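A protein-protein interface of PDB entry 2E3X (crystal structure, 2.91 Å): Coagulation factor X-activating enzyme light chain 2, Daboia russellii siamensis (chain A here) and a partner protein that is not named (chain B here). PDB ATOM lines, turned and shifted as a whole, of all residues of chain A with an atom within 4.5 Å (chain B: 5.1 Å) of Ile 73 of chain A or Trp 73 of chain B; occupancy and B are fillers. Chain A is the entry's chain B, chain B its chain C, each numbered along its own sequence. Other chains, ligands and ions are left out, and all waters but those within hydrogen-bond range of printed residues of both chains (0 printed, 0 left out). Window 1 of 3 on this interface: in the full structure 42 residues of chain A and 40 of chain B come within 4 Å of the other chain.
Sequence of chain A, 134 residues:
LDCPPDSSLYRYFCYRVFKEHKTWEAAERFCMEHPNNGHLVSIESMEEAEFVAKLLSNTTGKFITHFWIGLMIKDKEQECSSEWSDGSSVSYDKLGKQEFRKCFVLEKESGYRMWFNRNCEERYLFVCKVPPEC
Of chain B, only Trp 73, Cys 76 and Arg 77 come within 4 Å of Ile 73 of chain A. Trp 73 of chain B touches just these residues of chain A: Ile 73, Gln 78, Leu 95, Glu 99, Phe 100, Arg 101, Lys 102, Phe 104 and Asn 117. Printed residues of chain A within 4 Å of Cys 76 of chain B: Ile 73 (3.9 Å) and Cys 80 (2.0 Å). Printed residues of chain B within 4 Å of Arg 101 of chain A: Trp 73 (3.6 Å), Tyr 96 (3.1 Å) and Ser 109 (3.2 Å). Leu 91 of chain B touches none of the printed residues of chain A. The nearest residue of chain B that does not touch Ile 73 of chain A is Met 78 of chain B (4.5 Å). The nearest residue of chain A that does not touch Trp 73 of chain B is Cys 80 of chain A (4.02 Å).
Of the 12 printed residues of chain B, 9 touch a printed residue of chain A. Printed residues of chain B that touch a printed residue of chain A: Met 72, Trp 73, Lys 74, Cys 76, Arg 77, Met 78, Tyr 96, Leu 98 and Ser 109. Hydrophobic or aromatic side chains of chain B that line the printed part of chain A: Met 72, Trp 73, Met 78, Tyr 96 and Leu 98. Among the printed residues, 21 pairs touch across the chains. Among the printed residues, no Asp or Glu carboxylate lies within 4 Å of a Lys or Arg side-chain nitrogen of the other chain.
Among the printed residues, pairs that only touch across the chains: Met 72 of chain A with Met 78 of chain B, Ile 73 of chain A with Trp 73 of chain B, Ile 73 of chain A with Cys 76 of chain B, Ile 73 of chain A with Arg 77 of chain B, Gln 78 of chain A with Met 72 of chain B, Leu 95 of chain A with Trp 73 of chain B, Leu 95 of chain A with Leu 98 of chain B, Glu 99 of chain A with Trp 73 of chain B, Phe 100 of chain A with Trp 73 of chain B, Arg 101 of chain A with Trp 73 of chain B, Arg 101 of chain A with Tyr 96 of chain B, Lys 102 of chain A with Trp 73 of chain B, Phe 104 of chain A with Trp 73 of chain B, Asn 117 of chain A with Lys 74 of chain B and Asn 117 of chain A with Tyr 96 of chain B.
N of Lys 74 of chain A is in hydrogen-bond range of O of Arg 77 of chain B (2.9 Å). O of Gln 78 of chain A lies within hydrogen-bond range of NE1 of Trp 73 of chain B (2.8 Å). The side-chain sulfur of Cys 80 of chain A is disulfide-bonded to the side-chain sulfur of Cys 76 of chain B (2.0 Å). The backbone carbonyl oxygen of Glu 99 of chain A sits at hydrogen-bond distance from the side-chain hydroxyl of Ser 109 of chain B, 2.6 Å away. The guanidinium group of Arg 101 of chain A lies close to the side-chain hydroxyl of Ser 109 of chain B (3.3 Å). O of Trp 73 of chain B is in hydrogen-bond range of ND2 of Asn 117 of chain A.
The guanidinium group (NE) of Arg 101 of chain A sits close to the backbone carbonyl oxygen (O) of Glu 99 of chain A, at 3.2 Å. ND2 of Asn 117 of chain A is in hydrogen-bond range of O of Arg 101 of chain A (2.7 Å). The backbone carbonyl oxygen (O) of Tyr 96 of chain B lies within hydrogen-bond range of the backbone NH (N) of Asn 71 of chain B. The backbone carbonyl oxygen (O) of Tyr 96 of chain B is in hydrogen-bond range of the backbone NH (N) of Met 72 of chain B.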
ATOM      1  N   MET A  72      14.783 -18.187 -20.614  1.00  0.00           N
ATOM      2  CA  MET A  72      14.345 -18.996 -19.476  1.00  0.00           C
ATOM      3  C   MET A  72      14.834 -20.449 -19.535  1.00  0.00           C
ATOM      4  O   MET A  72      15.202 -20.947 -20.599  1.00  0.00           O
ATOM      5  CB  MET A  72      12.814 -18.948 -19.354  1.00  0.00           C
ATOM      6  CG  MET A  72      12.038 -19.500 -20.540  1.00  0.00           C
ATOM      7  SD  MET A  72      10.294 -18.956 -20.513  1.00  0.00           S
ATOM      8  CE  MET A  72       9.585 -20.064 -19.304  1.00  0.00           C
ATOM      9  N   ILE A  73      14.842 -21.123 -18.385  1.00  0.00           N
ATOM     10  CA  ILE A  73      15.305 -22.507 -18.304  1.00  0.00           C
ATOM     11  C   ILE A  73      14.181 -23.540 -18.265  1.00  0.00           C
ATOM     12  O   ILE A  73      13.124 -23.313 -17.674  1.00  0.00           O
ATOM     13  CB  ILE A  73      16.211 -22.723 -17.060  1.00  0.00           C
ATOM     14  CG1 ILE A  73      17.461 -21.845 -17.165  1.00  0.00           C
ATOM     15  CG2 ILE A  73      16.622 -24.185 -16.955  1.00  0.00           C
ATOM     16  CD1 ILE A  73      18.475 -22.071 -16.068  1.00  0.00           C
ATOM     17  N   LYS A  74      14.428 -24.683 -18.899  1.00  0.00           N
ATOM     18  CA  LYS A  74      13.463 -25.775 -18.950  1.00  0.00           C
ATOM     19  C   LYS A  74      13.920 -26.962 -18.095  1.00  0.00           C
ATOM     20  O   LYS A  74      14.865 -26.843 -17.319  1.00  0.00           O
ATOM     21  CB  LYS A  74      13.252 -26.210 -20.399  1.00  0.00           C
ATOM     22  CG  LYS A  74      12.801 -25.075 -21.310  1.00  0.00           C
ATOM     23  CD  LYS A  74      11.549 -24.407 -20.761  1.00  0.00           C
ATOM     24  CE  LYS A  74      11.052 -23.285 -21.658  1.00  0.00           C
ATOM     25  NZ  LYS A  74       9.806 -22.680 -21.101  1.00  0.00           N
ATOM     26  N   GLN A  78      16.668 -28.862 -10.935  1.00  0.00           N
ATOM     27  CA  GLN A  78      17.356 -27.689 -10.414  1.00  0.00           C
ATOM     28  C   GLN A  78      18.772 -27.619 -10.983  1.00  0.00           C
ATOM     29  O   GLN A  78      19.183 -26.598 -11.534  1.00  0.00           O
ATOM     30  CB  GLN A  78      17.396 -27.765  -8.884  1.00  0.00           C
ATOM     31  CG  GLN A  78      18.322 -26.777  -8.188  1.00  0.00           C
ATOM     32  CD  GLN A  78      19.789 -27.185  -8.240  1.00  0.00           C
ATOM     33  OE1 GLN A  78      20.520 -26.815  -9.159  1.00  0.00           O
ATOM     34  NE2 GLN A  78      20.221 -27.962  -7.251  1.00  0.00           N
ATOM     35  N   CYS A  80      19.775 -29.135 -13.455  1.00  0.00           N
ATOM     36  CA  CYS A  80      19.674 -29.345 -14.895  1.00  0.00           C
ATOM     37  C   CYS A  80      20.311 -30.674 -15.259  1.00  0.00           C
ATOM     38  O   CYS A  80      19.749 -31.735 -14.991  1.00  0.00           O
ATOM     39  CB  CYS A  80      20.372 -28.225 -15.666  1.00  0.00           C
ATOM     40  SG  CYS A  80      19.625 -26.578 -15.482  1.00  0.00           S
ATOM     41  N   LEU A  95      19.682 -27.505  -1.904  1.00  0.00           N
ATOM     42  CA  LEU A  95      19.894 -26.115  -2.273  1.00  0.00           C
ATOM     43  C   LEU A  95      18.551 -25.397  -2.170  1.00  0.00           C
ATOM     44  O   LEU A  95      17.631 -25.678  -2.939  1.00  0.00           O
ATOM     45  CB  LEU A  95      20.410 -26.014  -3.710  1.00  0.00           C
ATOM     46  CG  LEU A  95      20.734 -24.597  -4.194  1.00  0.00           C
ATOM     47  CD1 LEU A  95      22.053 -24.152  -3.585  1.00  0.00           C
ATOM     48  CD2 LEU A  95      20.827 -24.568  -5.703  1.00  0.00           C
ATOM     49  N   GLU A  99      18.054 -19.818  -3.674  1.00  0.00           N
ATOM     50  CA  GLU A  99      19.469 -19.798  -4.017  1.00  0.00           C
ATOM     51  C   GLU A  99      19.656 -19.982  -5.519  1.00  0.00           C
ATOM     52  O   GLU A  99      20.770 -19.879  -6.026  1.00  0.00           O
ATOM     53  CB  GLU A  99      20.210 -20.916  -3.282  1.00  0.00           C
ATOM     54  CG  GLU A  99      20.190 -20.800  -1.764  1.00  0.00           C
ATOM     55  CD  GLU A  99      20.834 -19.521  -1.267  1.00  0.00           C
ATOM     56  OE1 GLU A  99      22.015 -19.284  -1.607  1.00  0.00           O
ATOM     57  OE2 GLU A  99      20.158 -18.758  -0.539  1.00  0.00           O
ATOM     58  N   PHE A 100      18.565 -20.260  -6.227  1.00  0.00           N
ATOM     59  CA  PHE A 100      18.626 -20.473  -7.670  1.00  0.00           C
ATOM     60  C   PHE A 100      18.843 -19.155  -8.389  1.00  0.00           C
ATOM     61  O   PHE A 100      18.355 -18.113  -7.952  1.00  0.00           O
ATOM     62  CB  PHE A 100      17.319 -21.090  -8.189  1.00  0.00           C
ATOM     63  CG  PHE A 100      16.957 -22.418  -7.565  1.00  0.00           C
ATOM     64  CD1 PHE A 100      15.660 -22.916  -7.683  1.00  0.00           C
ATOM     65  CD2 PHE A 100      17.894 -23.169  -6.862  1.00  0.00           C
ATOM     66  CE1 PHE A 100      15.304 -24.134  -7.109  1.00  0.00           C
ATOM     67  CE2 PHE A 100      17.544 -24.393  -6.283  1.00  0.00           C
ATOM     68  CZ  PHE A 100      16.248 -24.874  -6.408  1.00  0.00           C
ATOM     69  N   ARG A 101      19.580 -19.212  -9.492  1.00  0.00           N
ATOM     70  CA  ARG A 101      19.852 -18.045 -10.329  1.00  0.00           C
ATOM     71  C   ARG A 101      19.576 -18.502 -11.759  1.00  0.00           C
ATOM     72  O   ARG A 101      20.485 -18.577 -12.587  1.00  0.00           O
ATOM     73  CB  ARG A 101      21.316 -17.597 -10.185  1.00  0.00           C
ATOM     74  CG  ARG A 101      21.608 -16.739  -8.954  1.00  0.00           C
ATOM     75  CD  ARG A 101      21.477 -17.543  -7.676  1.00  0.00           C
ATOM     76  NE  ARG A 101      20.926 -16.761  -6.570  1.00  0.00           N
ATOM     77  CZ  ARG A 101      21.564 -15.780  -5.943  1.00  0.00           C
ATOM     78  NH1 ARG A 101      22.798 -15.445  -6.302  1.00  0.00           N
ATOM     79  NH2 ARG A 101      20.961 -15.133  -4.954  1.00  0.00           N
ATOM     80  N   LYS A 102      18.311 -18.796 -12.049  1.00  0.00           N
ATOM     81  CA  LYS A 102      17.937 -19.308 -13.364  1.00  0.00           C
ATOM     82  C   LYS A 102      17.418 -18.329 -14.427  1.00  0.00           C
ATOM     83  O   LYS A 102      17.005 -18.751 -15.502  1.00  0.00           O
ATOM     84  CB  LYS A 102      16.960 -20.470 -13.167  1.00  0.00           C
ATOM     85  CG  LYS A 102      17.487 -21.478 -12.142  1.00  0.00           C
ATOM     86  CD  LYS A 102      16.542 -22.644 -11.872  1.00  0.00           C
ATOM     87  CE  LYS A 102      16.581 -23.675 -12.984  1.00  0.00           C
ATOM     88  NZ  LYS A 102      15.730 -24.858 -12.666  1.00  0.00           N
ATOM     89  N   PHE A 104      18.100 -14.463 -16.671  1.00  0.00           N
ATOM     90  CA  PHE A 104      19.248 -13.738 -17.202  1.00  0.00           C
ATOM     91  C   PHE A 104      18.987 -12.259 -17.462  1.00  0.00           C
ATOM     92  O   PHE A 104      17.889 -11.875 -17.855  1.00  0.00           O
ATOM     93  CB  PHE A 104      19.749 -14.413 -18.482  1.00  0.00           C
ATOM     94  CG  PHE A 104      20.068 -15.878 -18.314  1.00  0.00           C
ATOM     95  CD1 PHE A 104      19.058 -16.837 -18.352  1.00  0.00           C
ATOM     96  CD2 PHE A 104      21.375 -16.298 -18.104  1.00  0.00           C
ATOM     97  CE1 PHE A 104      19.349 -18.192 -18.182  1.00  0.00           C
ATOM     98  CE2 PHE A 104      21.675 -17.650 -17.932  1.00  0.00           C
ATOM     99  CZ  PHE A 104      20.662 -18.598 -17.971  1.00  0.00           C
ATOM    100  N   ASN A 117      23.452 -14.624 -14.833  1.00  0.00           N
ATOM    101  CA  ASN A 117      22.419 -15.309 -14.068  1.00  0.00           C
ATOM    102  C   ASN A 117      22.037 -14.429 -12.885  1.00  0.00           C
ATOM    103  O   ASN A 117      22.879 -13.734 -12.311  1.00  0.00           O
ATOM    104  CB  ASN A 117      22.916 -16.661 -13.544  1.00  0.00           C
ATOM    105  CG  ASN A 117      23.120 -17.693 -14.648  1.00  0.00           C
ATOM    106  OD1 ASN A 117      24.062 -17.607 -15.444  1.00  0.00           O
ATOM    107  ND2 ASN A 117      22.231 -18.680 -14.697  1.00  0.00           N
ATOM    108  N   ASN B  71      29.306 -23.860 -12.086  1.00  0.00           N
ATOM    109  CA  ASN B  71      28.711 -23.488 -13.359  1.00  0.00           C
ATOM    110  C   ASN B  71      27.352 -24.167 -13.353  1.00  0.00           C
ATOM    111  O   ASN B  71      27.055 -25.026 -14.188  1.00  0.00           O
ATOM    112  CB  ASN B  71      29.567 -24.014 -14.509  1.00  0.00           C
ATOM    113  CG  ASN B  71      31.038 -23.694 -14.328  1.00  0.00           C
ATOM    114  OD1 ASN B  71      31.427 -22.529 -14.250  1.00  0.00           O
ATOM    115  ND2 ASN B  71      31.865 -24.731 -14.258  1.00  0.00           N
ATOM    116  N   MET B  72      26.535 -23.768 -12.388  1.00  0.00           N
ATOM    117  CA  MET B  72      25.216 -24.338 -12.190  1.00  0.00           C
ATOM    118  C   MET B  72      24.146 -24.174 -13.262  1.00  0.00           C
ATOM    119  O   MET B  72      23.431 -25.134 -13.573  1.00  0.00           O
ATOM    120  CB  MET B  72      24.663 -23.860 -10.850  1.00  0.00           C
ATOM    121  CG  MET B  72      25.316 -24.551  -9.683  1.00  0.00           C
ATOM    122  SD  MET B  72      25.316 -26.332  -9.965  1.00  0.00           S
ATOM    123  CE  MET B  72      23.584 -26.728  -9.651  1.00  0.00           C
ATOM    124  N   TRP B  73      24.016 -22.984 -13.832  1.00  0.00           N
ATOM    125  CA  TRP B  73      22.978 -22.792 -14.833  1.00  0.00           C
ATOM    126  C   TRP B  73      23.509 -22.163 -16.106  1.00  0.00           C
ATOM    127  O   TRP B  73      23.037 -21.110 -16.537  1.00  0.00           O
ATOM    128  CB  TRP B  73      21.854 -21.960 -14.217  1.00  0.00           C
ATOM    129  CG  TRP B  73      21.354 -22.592 -12.939  1.00  0.00           C
ATOM    130  CD1 TRP B  73      20.569 -23.707 -12.828  1.00  0.00           C
ATOM    131  CD2 TRP B  73      21.713 -22.224 -11.600  1.00  0.00           C
ATOM    132  NE1 TRP B  73      20.427 -24.060 -11.508  1.00  0.00           N
ATOM    133  CE2 TRP B  73      21.119 -23.168 -10.733  1.00  0.00           C
ATOM    134  CE3 TRP B  73      22.485 -21.193 -11.049  1.00  0.00           C
ATOM    135  CZ2 TRP B  73      21.272 -23.110  -9.344  1.00  0.00           C
ATOM    136  CZ3 TRP B  73      22.637 -21.135  -9.671  1.00  0.00           C
ATOM    137  CH2 TRP B  73      22.032 -22.090  -8.832  1.00  0.00           C
ATOM    138  N   LYS B  74      24.488 -22.837 -16.710  1.00  0.00           N
ATOM    139  CA  LYS B  74      25.128 -22.375 -17.935  1.00  0.00           C
ATOM    140  C   LYS B  74      24.915 -23.350 -19.092  1.00  0.00           C
ATOM    141  O   LYS B  74      24.866 -22.943 -20.250  1.00  0.00           O
ATOM    142  CB  LYS B  74      26.634 -22.207 -17.710  1.00  0.00           C
ATOM    143  CG  LYS B  74      27.016 -21.435 -16.452  1.00  0.00           C
ATOM    144  CD  LYS B  74      26.700 -19.950 -16.562  1.00  0.00           C
ATOM    145  CE  LYS B  74      27.680 -19.235 -17.469  1.00  0.00           C
ATOM    146  NZ  LYS B  74      27.374 -17.781 -17.561  1.00  0.00           N
ATOM    147  N   ASP B  75      24.798 -24.636 -18.775  1.00  0.00           N
ATOM    148  CA  ASP B  75      24.609 -25.669 -19.795  1.00  0.00           C
ATOM    149  C   ASP B  75      23.253 -26.368 -19.710  1.00  0.00           C
ATOM    150  O   ASP B  75      23.166 -27.582 -19.899  1.00  0.00           O
ATOM    151  CB  ASP B  75      25.715 -26.720 -19.673  1.00  0.00           C
ATOM    152  CG  ASP B  75      27.093 -26.153 -19.934  1.00  0.00           C
ATOM    153  OD1 ASP B  75      27.396 -25.835 -21.104  1.00  0.00           O
ATOM    154  OD2 ASP B  75      27.874 -26.020 -18.968  1.00  0.00           O
ATOM    155  N   CYS B  76      22.200 -25.606 -19.427  1.00  0.00           N
ATOM    156  CA  CYS B  76      20.854 -26.164 -19.313  1.00  0.00           C
ATOM    157  C   CYS B  76      20.095 -26.071 -20.632  1.00  0.00           C
ATOM    158  O   CYS B  76      20.580 -25.469 -21.586  1.00  0.00           O
ATOM    159  CB  CYS B  76      20.067 -25.410 -18.245  1.00  0.00           C
ATOM    160  SG  CYS B  76      20.837 -25.389 -16.597  1.00  0.00           S
ATOM    161  N   ARG B  77      18.910 -26.676 -20.682  1.00  0.00           N
ATOM    162  CA  ARG B  77      18.079 -26.612 -21.881  1.00  0.00           C
ATOM    163  C   ARG B  77      17.292 -25.322 -21.739  1.00  0.00           C
ATOM    164  O   ARG B  77      16.564 -25.144 -20.766  1.00  0.00           O
ATOM    165  CB  ARG B  77      17.115 -27.799 -21.960  1.00  0.00           C
ATOM    166  CG  ARG B  77      17.799 -29.140 -21.833  1.00  0.00           C
ATOM    167  CD  ARG B  77      17.046 -30.250 -22.546  1.00  0.00           C
ATOM    168  NE  ARG B  77      17.723 -31.533 -22.357  1.00  0.00           N
ATOM    169  CZ  ARG B  77      17.753 -32.510 -23.257  1.00  0.00           C
ATOM    170  NH1 ARG B  77      17.143 -32.361 -24.427  1.00  0.00           N
ATOM    171  NH2 ARG B  77      18.401 -33.637 -22.990  1.00  0.00           N
ATOM    172  N   MET B  78      17.442 -24.418 -22.697  1.00  0.00           N
ATOM    173  CA  MET B  78      16.748 -23.144 -22.622  1.00  0.00           C
ATOM    174  C   MET B  78      15.803 -22.898 -23.790  1.00  0.00           C
ATOM    175  O   MET B  78      15.656 -23.738 -24.675  1.00  0.00           O
ATOM    176  CB  MET B  78      17.773 -22.017 -22.541  1.00  0.00           C
ATOM    177  CG  MET B  78      18.775 -22.191 -21.420  1.00  0.00           C
ATOM    178  SD  MET B  78      20.006 -20.887 -21.405  1.00  0.00           S
ATOM    179  CE  MET B  78      21.184 -21.517 -22.630  1.00  0.00           C
ATOM    180  N   LEU B  91      26.375 -16.032 -22.966  1.00  0.00           N
ATOM    181  CA  LEU B  91      26.485 -16.172 -21.515  1.00  0.00           C
ATOM    182  C   LEU B  91      27.778 -15.586 -20.964  1.00  0.00           C
ATOM    183  O   LEU B  91      28.871 -15.966 -21.382  1.00  0.00           O
ATOM    184  CB  LEU B  91      26.385 -17.649 -21.116  1.00  0.00           C
ATOM    185  CG  LEU B  91      24.984 -18.229 -20.898  1.00  0.00           C
ATOM    186  CD1 LEU B  91      24.127 -17.981 -22.113  1.00  0.00           C
ATOM    187  CD2 LEU B  91      25.086 -19.713 -20.615  1.00  0.00           C
ATOM    188  N   TYR B  96      27.911 -19.317 -11.269  1.00  0.00           N
ATOM    189  CA  TYR B  96      27.665 -19.712  -9.889  1.00  0.00           C
ATOM    190  C   TYR B  96      28.095 -21.119  -9.501  1.00  0.00           C
ATOM    191  O   TYR B  96      28.025 -22.061 -10.295  1.00  0.00           O
ATOM    192  CB  TYR B  96      26.184 -19.539  -9.545  1.00  0.00           C
ATOM    193  CG  TYR B  96      25.789 -18.102  -9.350  1.00  0.00           C
ATOM    194  CD1 TYR B  96      25.576 -17.261 -10.439  1.00  0.00           C
ATOM    195  CD2 TYR B  96      25.680 -17.563  -8.071  1.00  0.00           C
ATOM    196  CE1 TYR B  96      25.268 -15.911 -10.253  1.00  0.00           C
ATOM    197  CE2 TYR B  96      25.374 -16.219  -7.877  1.00  0.00           C
ATOM    198  CZ  TYR B  96      25.171 -15.402  -8.968  1.00  0.00           C
ATOM    199  OH  TYR B  96      24.883 -14.075  -8.773  1.00  0.00           O
ATOM    200  N   LEU B  98      28.284 -23.886  -5.802  1.00  0.00           N
ATOM    201  CA  LEU B  98      27.637 -24.152  -4.522  1.00  0.00           C
ATOM    202  C   LEU B  98      28.595 -24.202  -3.341  1.00  0.00           C
ATOM    203  O   LEU B  98      29.714 -24.703  -3.446  1.00  0.00           O
ATOM    204  CB  LEU B  98      26.848 -25.462  -4.600  1.00  0.00           C
ATOM    205  CG  LEU B  98      25.384 -25.391  -5.050  1.00  0.00           C
ATOM    206  CD1 LEU B  98      25.221 -24.490  -6.258  1.00  0.00           C
ATOM    207  CD2 LEU B  98      24.906 -26.794  -5.357  1.00  0.00           C
ATOM    208  N   SER B 109      24.300 -20.395  -3.153  1.00  0.00           N
ATOM    209  CA  SER B 109      24.934 -20.232  -4.451  1.00  0.00           C
ATOM    210  C   SER B 109      25.827 -19.003  -4.329  1.00  0.00           C
ATOM    211  O   SER B 109      25.453 -18.006  -3.706  1.00  0.00           O
ATOM    212  CB  SER B 109      23.885 -20.040  -5.557  1.00  0.00           C
ATOM    213  OG  SER B 109      23.058 -18.914  -5.312  1.00  0.00           O
